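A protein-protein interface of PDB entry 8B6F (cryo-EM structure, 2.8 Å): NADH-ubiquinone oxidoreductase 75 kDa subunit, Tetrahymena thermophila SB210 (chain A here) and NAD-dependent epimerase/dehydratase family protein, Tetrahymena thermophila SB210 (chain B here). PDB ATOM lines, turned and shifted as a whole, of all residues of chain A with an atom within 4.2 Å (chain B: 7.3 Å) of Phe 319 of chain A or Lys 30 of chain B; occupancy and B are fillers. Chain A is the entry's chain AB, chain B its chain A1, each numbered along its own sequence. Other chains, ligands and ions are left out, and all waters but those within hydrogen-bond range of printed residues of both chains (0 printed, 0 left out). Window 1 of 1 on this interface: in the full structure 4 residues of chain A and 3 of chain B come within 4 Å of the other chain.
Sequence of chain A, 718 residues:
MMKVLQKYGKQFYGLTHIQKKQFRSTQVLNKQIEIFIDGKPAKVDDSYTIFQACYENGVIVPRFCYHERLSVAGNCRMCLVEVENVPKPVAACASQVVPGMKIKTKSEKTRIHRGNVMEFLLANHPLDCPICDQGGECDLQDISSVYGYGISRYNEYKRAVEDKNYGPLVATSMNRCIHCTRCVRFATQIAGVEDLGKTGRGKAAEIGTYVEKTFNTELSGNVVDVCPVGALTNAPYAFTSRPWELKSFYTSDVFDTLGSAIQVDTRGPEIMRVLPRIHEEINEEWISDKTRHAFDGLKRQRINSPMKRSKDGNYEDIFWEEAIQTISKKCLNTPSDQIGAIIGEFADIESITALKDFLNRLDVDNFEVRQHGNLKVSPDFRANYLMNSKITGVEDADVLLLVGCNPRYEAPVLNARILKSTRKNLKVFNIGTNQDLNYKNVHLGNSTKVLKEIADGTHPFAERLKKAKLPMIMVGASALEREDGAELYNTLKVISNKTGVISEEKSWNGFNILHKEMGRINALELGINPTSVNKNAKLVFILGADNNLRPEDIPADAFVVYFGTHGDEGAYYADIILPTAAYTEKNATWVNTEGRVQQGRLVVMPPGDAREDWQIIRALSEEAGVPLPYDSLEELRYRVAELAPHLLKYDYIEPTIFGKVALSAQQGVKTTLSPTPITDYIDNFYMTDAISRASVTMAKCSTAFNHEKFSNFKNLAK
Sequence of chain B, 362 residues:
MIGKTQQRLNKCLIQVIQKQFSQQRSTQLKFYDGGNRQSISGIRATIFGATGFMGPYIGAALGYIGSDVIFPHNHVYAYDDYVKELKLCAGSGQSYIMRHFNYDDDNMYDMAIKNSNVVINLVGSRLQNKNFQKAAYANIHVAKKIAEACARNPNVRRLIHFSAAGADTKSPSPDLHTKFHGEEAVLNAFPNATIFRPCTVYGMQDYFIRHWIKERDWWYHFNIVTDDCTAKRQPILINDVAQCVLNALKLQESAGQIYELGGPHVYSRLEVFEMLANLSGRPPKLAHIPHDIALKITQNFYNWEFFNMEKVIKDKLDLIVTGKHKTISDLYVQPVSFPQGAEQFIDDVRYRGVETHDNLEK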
ATOM      1  N   ILE A 318      12.881  15.986 -22.164  1.00  0.00           N
ATOM      2  CA  ILE A 318      14.071  15.890 -21.331  1.00  0.00           C
ATOM      3  C   ILE A 318      14.826  14.624 -21.714  1.00  0.00           C
ATOM      4  O   ILE A 318      14.334  13.778 -22.460  1.00  0.00           O
ATOM      5  CB  ILE A 318      13.736  15.887 -19.823  1.00  0.00           C
ATOM      6  CG1 ILE A 318      12.788  14.731 -19.485  1.00  0.00           C
ATOM      7  CG2 ILE A 318      13.125  17.218 -19.429  1.00  0.00           C
ATOM      8  CD1 ILE A 318      12.465  14.597 -18.005  1.00  0.00           C
ATOM      9  N   PHE A 319      16.042  14.507 -21.189  1.00  0.00           N
ATOM     10  CA  PHE A 319      16.875  13.345 -21.443  1.00  0.00           C
ATOM     11  C   PHE A 319      16.472  12.182 -20.541  1.00  0.00           C
ATOM     12  O   PHE A 319      15.885  12.360 -19.471  1.00  0.00           O
ATOM     13  CB  PHE A 319      18.350  13.677 -21.221  1.00  0.00           C
ATOM     14  CG  PHE A 319      18.955  14.500 -22.317  1.00  0.00           C
ATOM     15  CD1 PHE A 319      18.918  15.882 -22.265  1.00  0.00           C
ATOM     16  CD2 PHE A 319      19.568  13.889 -23.396  1.00  0.00           C
ATOM     17  CE1 PHE A 319      19.479  16.640 -23.274  1.00  0.00           C
ATOM     18  CE2 PHE A 319      20.130  14.640 -24.407  1.00  0.00           C
ATOM     19  CZ  PHE A 319      20.085  16.017 -24.347  1.00  0.00           C
ATOM     20  N   TRP A 320      16.798  10.970 -20.995  1.00  0.00           N
ATOM     21  CA  TRP A 320      16.555   9.790 -20.173  1.00  0.00           C
ATOM     22  C   TRP A 320      17.286   9.893 -18.842  1.00  0.00           C
ATOM     23  O   TRP A 320      16.746   9.515 -17.796  1.00  0.00           O
ATOM     24  CB  TRP A 320      16.987   8.529 -20.919  1.00  0.00           C
ATOM     25  CG  TRP A 320      15.995   8.058 -21.924  1.00  0.00           C
ATOM     26  CD1 TRP A 320      16.043   8.241 -23.273  1.00  0.00           C
ATOM     27  CD2 TRP A 320      14.800   7.316 -21.661  1.00  0.00           C
ATOM     28  NE1 TRP A 320      14.951   7.659 -23.868  1.00  0.00           N
ATOM     29  CE2 TRP A 320      14.172   7.084 -22.899  1.00  0.00           C
ATOM     30  CE3 TRP A 320      14.201   6.825 -20.496  1.00  0.00           C
ATOM     31  CZ2 TRP A 320      12.974   6.384 -23.007  1.00  0.00           C
ATOM     32  CZ3 TRP A 320      13.010   6.128 -20.605  1.00  0.00           C
ATOM     33  CH2 TRP A 320      12.409   5.914 -21.852  1.00  0.00           C
ATOM     34  N   GLU A 321      18.515  10.410 -18.859  1.00  0.00           N
ATOM     35  CA  GLU A 321      19.276  10.543 -17.622  1.00  0.00           C
ATOM     36  C   GLU A 321      18.551  11.452 -16.638  1.00  0.00           C
ATOM     37  O   GLU A 321      18.410  11.119 -15.456  1.00  0.00           O
ATOM     38  CB  GLU A 321      20.678  11.076 -17.924  1.00  0.00           C
ATOM     39  CG  GLU A 321      21.593  11.126 -16.709  1.00  0.00           C
ATOM     40  CD  GLU A 321      23.024  11.481 -17.069  1.00  0.00           C
ATOM     41  OE1 GLU A 321      23.316  11.628 -18.274  1.00  0.00           O
ATOM     42  OE2 GLU A 321      23.857  11.613 -16.148  1.00  0.00           O
ATOM     43  N   GLU A 322      18.078  12.606 -17.108  1.00  0.00           N
ATOM     44  CA  GLU A 322      17.373  13.522 -16.219  1.00  0.00           C
ATOM     45  C   GLU A 322      16.100  12.882 -15.681  1.00  0.00           C
ATOM     46  O   GLU A 322      15.806  12.969 -14.484  1.00  0.00           O
ATOM     47  CB  GLU A 322      17.051  14.823 -16.953  1.00  0.00           C
ATOM     48  CG  GLU A 322      16.277  15.826 -16.109  1.00  0.00           C
ATOM     49  CD  GLU A 322      15.968  17.103 -16.861  1.00  0.00           C
ATOM     50  OE1 GLU A 322      16.423  17.237 -18.016  1.00  0.00           O
ATOM     51  OE2 GLU A 322      15.267  17.970 -16.300  1.00  0.00           O
ATOM     52  N   ALA A 323      15.325  12.239 -16.555  1.00  0.00           N
ATOM     53  CA  ALA A 323      14.070  11.630 -16.127  1.00  0.00           C
ATOM     54  C   ALA A 323      14.314  10.543 -15.087  1.00  0.00           C
ATOM     55  O   ALA A 323      13.618  10.471 -14.069  1.00  0.00           O
ATOM     56  CB  ALA A 323      13.325  11.061 -17.335  1.00  0.00           C
ATOM     57  N   ASP A 609      13.102   7.903 -29.518  1.00  0.00           N
ATOM     58  CA  ASP A 609      13.986   7.600 -28.401  1.00  0.00           C
ATOM     59  C   ASP A 609      13.368   6.603 -27.428  1.00  0.00           C
ATOM     60  O   ASP A 609      13.848   6.469 -26.298  1.00  0.00           O
ATOM     61  CB  ASP A 609      14.358   8.888 -27.668  1.00  0.00           C
ATOM     62  CG  ASP A 609      15.665   8.771 -26.908  1.00  0.00           C
ATOM     63  OD1 ASP A 609      16.087   7.634 -26.616  1.00  0.00           O
ATOM     64  OD2 ASP A 609      16.272   9.818 -26.605  1.00  0.00           O
ATOM     65  N   THR B  27      18.313  25.175 -24.499  1.00  0.00           N
ATOM     66  CA  THR B  27      19.608  24.887 -25.098  1.00  0.00           C
ATOM     67  C   THR B  27      19.858  23.396 -25.278  1.00  0.00           C
ATOM     68  O   THR B  27      20.946  23.015 -25.716  1.00  0.00           O
ATOM     69  CB  THR B  27      20.731  25.495 -24.250  1.00  0.00           C
ATOM     70  OG1 THR B  27      20.636  25.014 -22.903  1.00  0.00           O
ATOM     71  CG2 THR B  27      20.646  27.012 -24.256  1.00  0.00           C
ATOM     72  N   GLN B  28      18.885  22.549 -24.952  1.00  0.00           N
ATOM     73  CA  GLN B  28      19.083  21.113 -25.072  1.00  0.00           C
ATOM     74  C   GLN B  28      19.240  20.717 -26.534  1.00  0.00           C
ATOM     75  O   GLN B  28      18.618  21.294 -27.430  1.00  0.00           O
ATOM     76  CB  GLN B  28      17.914  20.350 -24.451  1.00  0.00           C
ATOM     77  CG  GLN B  28      16.589  20.541 -25.170  1.00  0.00           C
ATOM     78  CD  GLN B  28      15.499  19.645 -24.616  1.00  0.00           C
ATOM     79  OE1 GLN B  28      15.722  18.884 -23.675  1.00  0.00           O
ATOM     80  NE2 GLN B  28      14.309  19.730 -25.202  1.00  0.00           N
ATOM     81  N   LEU B  29      20.084  19.716 -26.769  1.00  0.00           N
ATOM     82  CA  LEU B  29      20.360  19.221 -28.113  1.00  0.00           C
ATOM     83  C   LEU B  29      20.387  17.701 -28.053  1.00  0.00           C
ATOM     84  O   LEU B  29      21.339  17.116 -27.526  1.00  0.00           O
ATOM     85  CB  LEU B  29      21.682  19.777 -28.645  1.00  0.00           C
ATOM     86  CG  LEU B  29      21.992  19.510 -30.119  1.00  0.00           C
ATOM     87  CD1 LEU B  29      21.007  20.237 -31.018  1.00  0.00           C
ATOM     88  CD2 LEU B  29      23.417  19.917 -30.445  1.00  0.00           C
ATOM     89  N   LYS B  30      19.348  17.065 -28.586  1.00  0.00           N
ATOM     90  CA  LYS B  30      19.243  15.610 -28.608  1.00  0.00           C
ATOM     91  C   LYS B  30      19.789  15.106 -29.938  1.00  0.00           C
ATOM     92  O   LYS B  30      19.163  15.297 -30.985  1.00  0.00           O
ATOM     93  CB  LYS B  30      17.793  15.173 -28.417  1.00  0.00           C
ATOM     94  CG  LYS B  30      17.529  14.391 -27.141  1.00  0.00           C
ATOM     95  CD  LYS B  30      16.053  14.025 -27.027  1.00  0.00           C
ATOM     96  CE  LYS B  30      15.763  13.227 -25.766  1.00  0.00           C
ATOM     97  NZ  LYS B  30      16.471  11.918 -25.751  1.00  0.00           N
ATOM     98  N   PHE B  31      20.954  14.464 -29.901  1.00  0.00           N
ATOM     99  CA  PHE B  31      21.552  13.903 -31.102  1.00  0.00           C
ATOM    100  C   PHE B  31      22.230  12.585 -30.761  1.00  0.00           C
ATOM    101  O   PHE B  31      22.648  12.356 -29.624  1.00  0.00           O
ATOM    102  CB  PHE B  31      22.556  14.871 -31.746  1.00  0.00           C
ATOM    103  CG  PHE B  31      23.835  15.033 -30.976  1.00  0.00           C
ATOM    104  CD1 PHE B  31      23.921  15.936 -29.932  1.00  0.00           C
ATOM    105  CD2 PHE B  31      24.958  14.300 -31.317  1.00  0.00           C
ATOM    106  CE1 PHE B  31      25.101  16.094 -29.231  1.00  0.00           C
ATOM    107  CE2 PHE B  31      26.140  14.453 -30.621  1.00  0.00           C
ATOM    108  CZ  PHE B  31      26.211  15.351 -29.576  1.00  0.00           C
ATOM    109  N   TYR B  32      22.323  11.717 -31.765  1.00  0.00           N
ATOM    110  CA  TYR B  32      22.909  10.390 -31.629  1.00  0.00           C
ATOM    111  C   TYR B  32      24.281  10.394 -32.288  1.00  0.00           C
ATOM    112  O   TYR B  32      24.394  10.649 -33.492  1.00  0.00           O
ATOM    113  CB  TYR B  32      22.000   9.339 -32.267  1.00  0.00           C
ATOM    114  CG  TYR B  32      22.564   7.940 -32.259  1.00  0.00           C
ATOM    115  CD1 TYR B  32      22.727   7.241 -31.072  1.00  0.00           C
ATOM    116  CD2 TYR B  32      22.911   7.308 -33.445  1.00  0.00           C
ATOM    117  CE1 TYR B  32      23.235   5.958 -31.063  1.00  0.00           C
ATOM    118  CE2 TYR B  32      23.419   6.026 -33.448  1.00  0.00           C
ATOM    119  CZ  TYR B  32      23.577   5.355 -32.256  1.00  0.00           C
ATOM    120  OH  TYR B  32      24.083   4.076 -32.257  1.00  0.00           O
ATOM    121  N   SER B  41      22.383  12.012 -37.348  1.00  0.00           N
ATOM    122  CA  SER B  41      22.885  12.485 -36.063  1.00  0.00           C
ATOM    123  C   SER B  41      21.804  13.215 -35.279  1.00  0.00           C
ATOM    124  O   SER B  41      21.671  13.026 -34.065  1.00  0.00           O
ATOM    125  CB  SER B  41      24.085  13.405 -36.283  1.00  0.00           C
ATOM    126  OG  SER B  41      24.561  13.920 -35.053  1.00  0.00           O
ATOM    127  N   GLY B  42      21.017  14.040 -35.956  1.00  0.00           N
ATOM    128  CA  GLY B  42      20.079  14.922 -35.299  1.00  0.00           C
ATOM    129  C   GLY B  42      20.562  16.345 -35.142  1.00  0.00           C
ATOM    130  O   GLY B  42      19.878  17.143 -34.492  1.00  0.00           O
ATOM    131  N   ILE B  43      21.711  16.687 -35.716  1.00  0.00           N
ATOM    132  CA  ILE B  43      22.251  18.040 -35.685  1.00  0.00           C
ATOM    133  C   ILE B  43      22.134  18.626 -37.083  1.00  0.00           C
ATOM    134  O   ILE B  43      22.595  18.021 -38.058  1.00  0.00           O
ATOM    135  CB  ILE B  43      23.713  18.061 -35.206  1.00  0.00           C
ATOM    136  CG1 ILE B  43      23.813  17.517 -33.779  1.00  0.00           C
ATOM    137  CG2 ILE B  43      24.274  19.477 -35.282  1.00  0.00           C
ATOM    138  CD1 ILE B  43      25.234  17.392 -33.263  1.00  0.00           C
ATOM    139  N   ASN B 117      19.860  24.036 -36.075  1.00  0.00           N
ATOM    140  CA  ASN B 117      19.813  24.159 -34.626  1.00  0.00           C
ATOM    141  C   ASN B 117      21.188  24.401 -34.014  1.00  0.00           C
ATOM    142  O   ASN B 117      21.276  24.654 -32.809  1.00  0.00           O
ATOM    143  CB  ASN B 117      19.182  22.907 -34.004  1.00  0.00           C
ATOM    144  CG  ASN B 117      19.827  21.623 -34.487  1.00  0.00           C
ATOM    145  OD1 ASN B 117      20.959  21.625 -34.966  1.00  0.00           O
ATOM    146  ND2 ASN B 117      19.103  20.518 -34.366  1.00  0.00           N
ATOM    147  N   ARG B 157      19.362  26.110 -31.333  1.00  0.00           N
ATOM    148  CA  ARG B 157      19.589  25.695 -29.954  1.00  0.00           C
ATOM    149  C   ARG B 157      20.949  26.154 -29.441  1.00  0.00           C
ATOM    150  O   ARG B 157      21.058  26.623 -28.302  1.00  0.00           O
ATOM    151  CB  ARG B 157      19.464  24.176 -29.839  1.00  0.00           C
ATOM    152  CG  ARG B 157      18.094  23.637 -30.223  1.00  0.00           C
ATOM    153  CD  ARG B 157      17.001  24.197 -29.328  1.00  0.00           C
ATOM    154  NE  ARG B 157      15.704  23.593 -29.606  1.00  0.00           N
ATOM    155  CZ  ARG B 157      15.278  22.454 -29.079  1.00  0.00           C
ATOM    156  NH1 ARG B 157      16.026  21.756 -28.241  1.00  0.00           N
ATOM    157  NH2 ARG B 157      14.070  22.001 -29.402  1.00  0.00           N
ATOM    158  N   LEU B 249      28.992  20.656 -27.454  1.00  0.00           N
ATOM    159  CA  LEU B 249      27.625  20.404 -27.898  1.00  0.00           C
ATOM    160  C   LEU B 249      26.932  19.395 -26.990  1.00  0.00           C
ATOM    161  O   LEU B 249      25.750  19.550 -26.665  1.00  0.00           O
ATOM    162  CB  LEU B 249      27.633  19.911 -29.345  1.00  0.00           C
ATOM    163  CG  LEU B 249      28.004  20.947 -30.411  1.00  0.00           C
ATOM    164  CD1 LEU B 249      28.124  20.286 -31.770  1.00  0.00           C
ATOM    165  CD2 LEU B 249      26.991  22.078 -30.463  1.00  0.00           C
ATOM    166  N   LYS B 250      27.651  18.349 -26.576  1.00  0.00           N
ATOM    167  CA  LYS B 250      27.058  17.347 -25.697  1.00  0.00           C
ATOM    168  C   LYS B 250      26.688  17.945 -24.346  1.00  0.00           C
ATOM    169  O   LYS B 250      25.649  17.603 -23.770  1.00  0.00           O
ATOM    170  CB  LYS B 250      28.023  16.175 -25.512  1.00  0.00           C
ATOM    171  CG  LYS B 250      28.215  15.320 -26.753  1.00  0.00           C
ATOM    172  CD  LYS B 250      29.220  14.207 -26.505  1.00  0.00           C
ATOM    173  CE  LYS B 250      29.413  13.349 -27.744  1.00  0.00           C
ATOM    174  NZ  LYS B 250      30.410  12.265 -27.517  1.00  0.00           N
ATOM    175  N   GLN B 252      25.236  20.521 -22.024  1.00  0.00           N
ATOM    176  CA  GLN B 252      24.301  21.639 -22.079  1.00  0.00           C
ATOM    177  C   GLN B 252      24.800  22.818 -21.252  1.00  0.00           C
ATOM    178  O   GLN B 252      24.622  23.976 -21.644  1.00  0.00           O
ATOM    179  CB  GLN B 252      22.922  21.187 -21.598  1.00  0.00           C
ATOM    180  CG  GLN B 252      21.835  22.244 -21.725  1.00  0.00           C
ATOM    181  CD  GLN B 252      20.482  21.733 -21.272  1.00  0.00           C
ATOM    182  OE1 GLN B 252      20.347  20.582 -20.861  1.00  0.00           O
ATOM    183  NE2 GLN B 252      19.471  22.592 -21.341  1.00  0.00           N
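OD2 of Asp 609 of chain A lies close to NZ of Lys 30 of chain B, at 2.3 Å.
The indole nitrogen (NE1) of Trp 320 of chain A sits at hydrogen-bond distance from the backbone carbonyl oxygen (O) of Asp 609 of chain A, at 2.9 Å.
O of Ile 318 of chain A touches CE of Lys 30 of chain B, at 3.6 Å. Phe 319 of chain A touches Leu 29 of chain B. Lys 30 of chain B touches Phe 319 of chain A.
Of the printed residues of chain B, Ile 318 of chain A touches Lys 30. Printed residues of chain B within 4 Å of Phe 319 of chain A: Leu 29 and Lys 30. Ala 323 of chain A touches none of the printed residues of chain B. Printed residues of chain A within 4 Å of Leu 29 of chain B: Phe 319. Lys 30 of chain B touches just these residues of chain A: Ile 318, Phe 319 and Asp 609. The nearest residue of chain B that does not touch Phe 319 of chain A is Gln 28 of chain B (4.2 Å).
Hydrophobic or aromatic side chains of chain A within 4 Å of the printed part of chain B: Phe 319. Of the 14 printed residues of chain B, 2 touch a printed residue of chain A. Printed residues of chain B that touch a printed residue of chain A: Leu 29 and Lys 30. Among the printed residues, 4 pairs touch across the chains. Among the printed residues, Asp or Glu carboxylates within 4 Å of a Lys or Arg side-chain nitrogen of the other chain: Asp 609 of chain A with Lys 30 of chain B.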
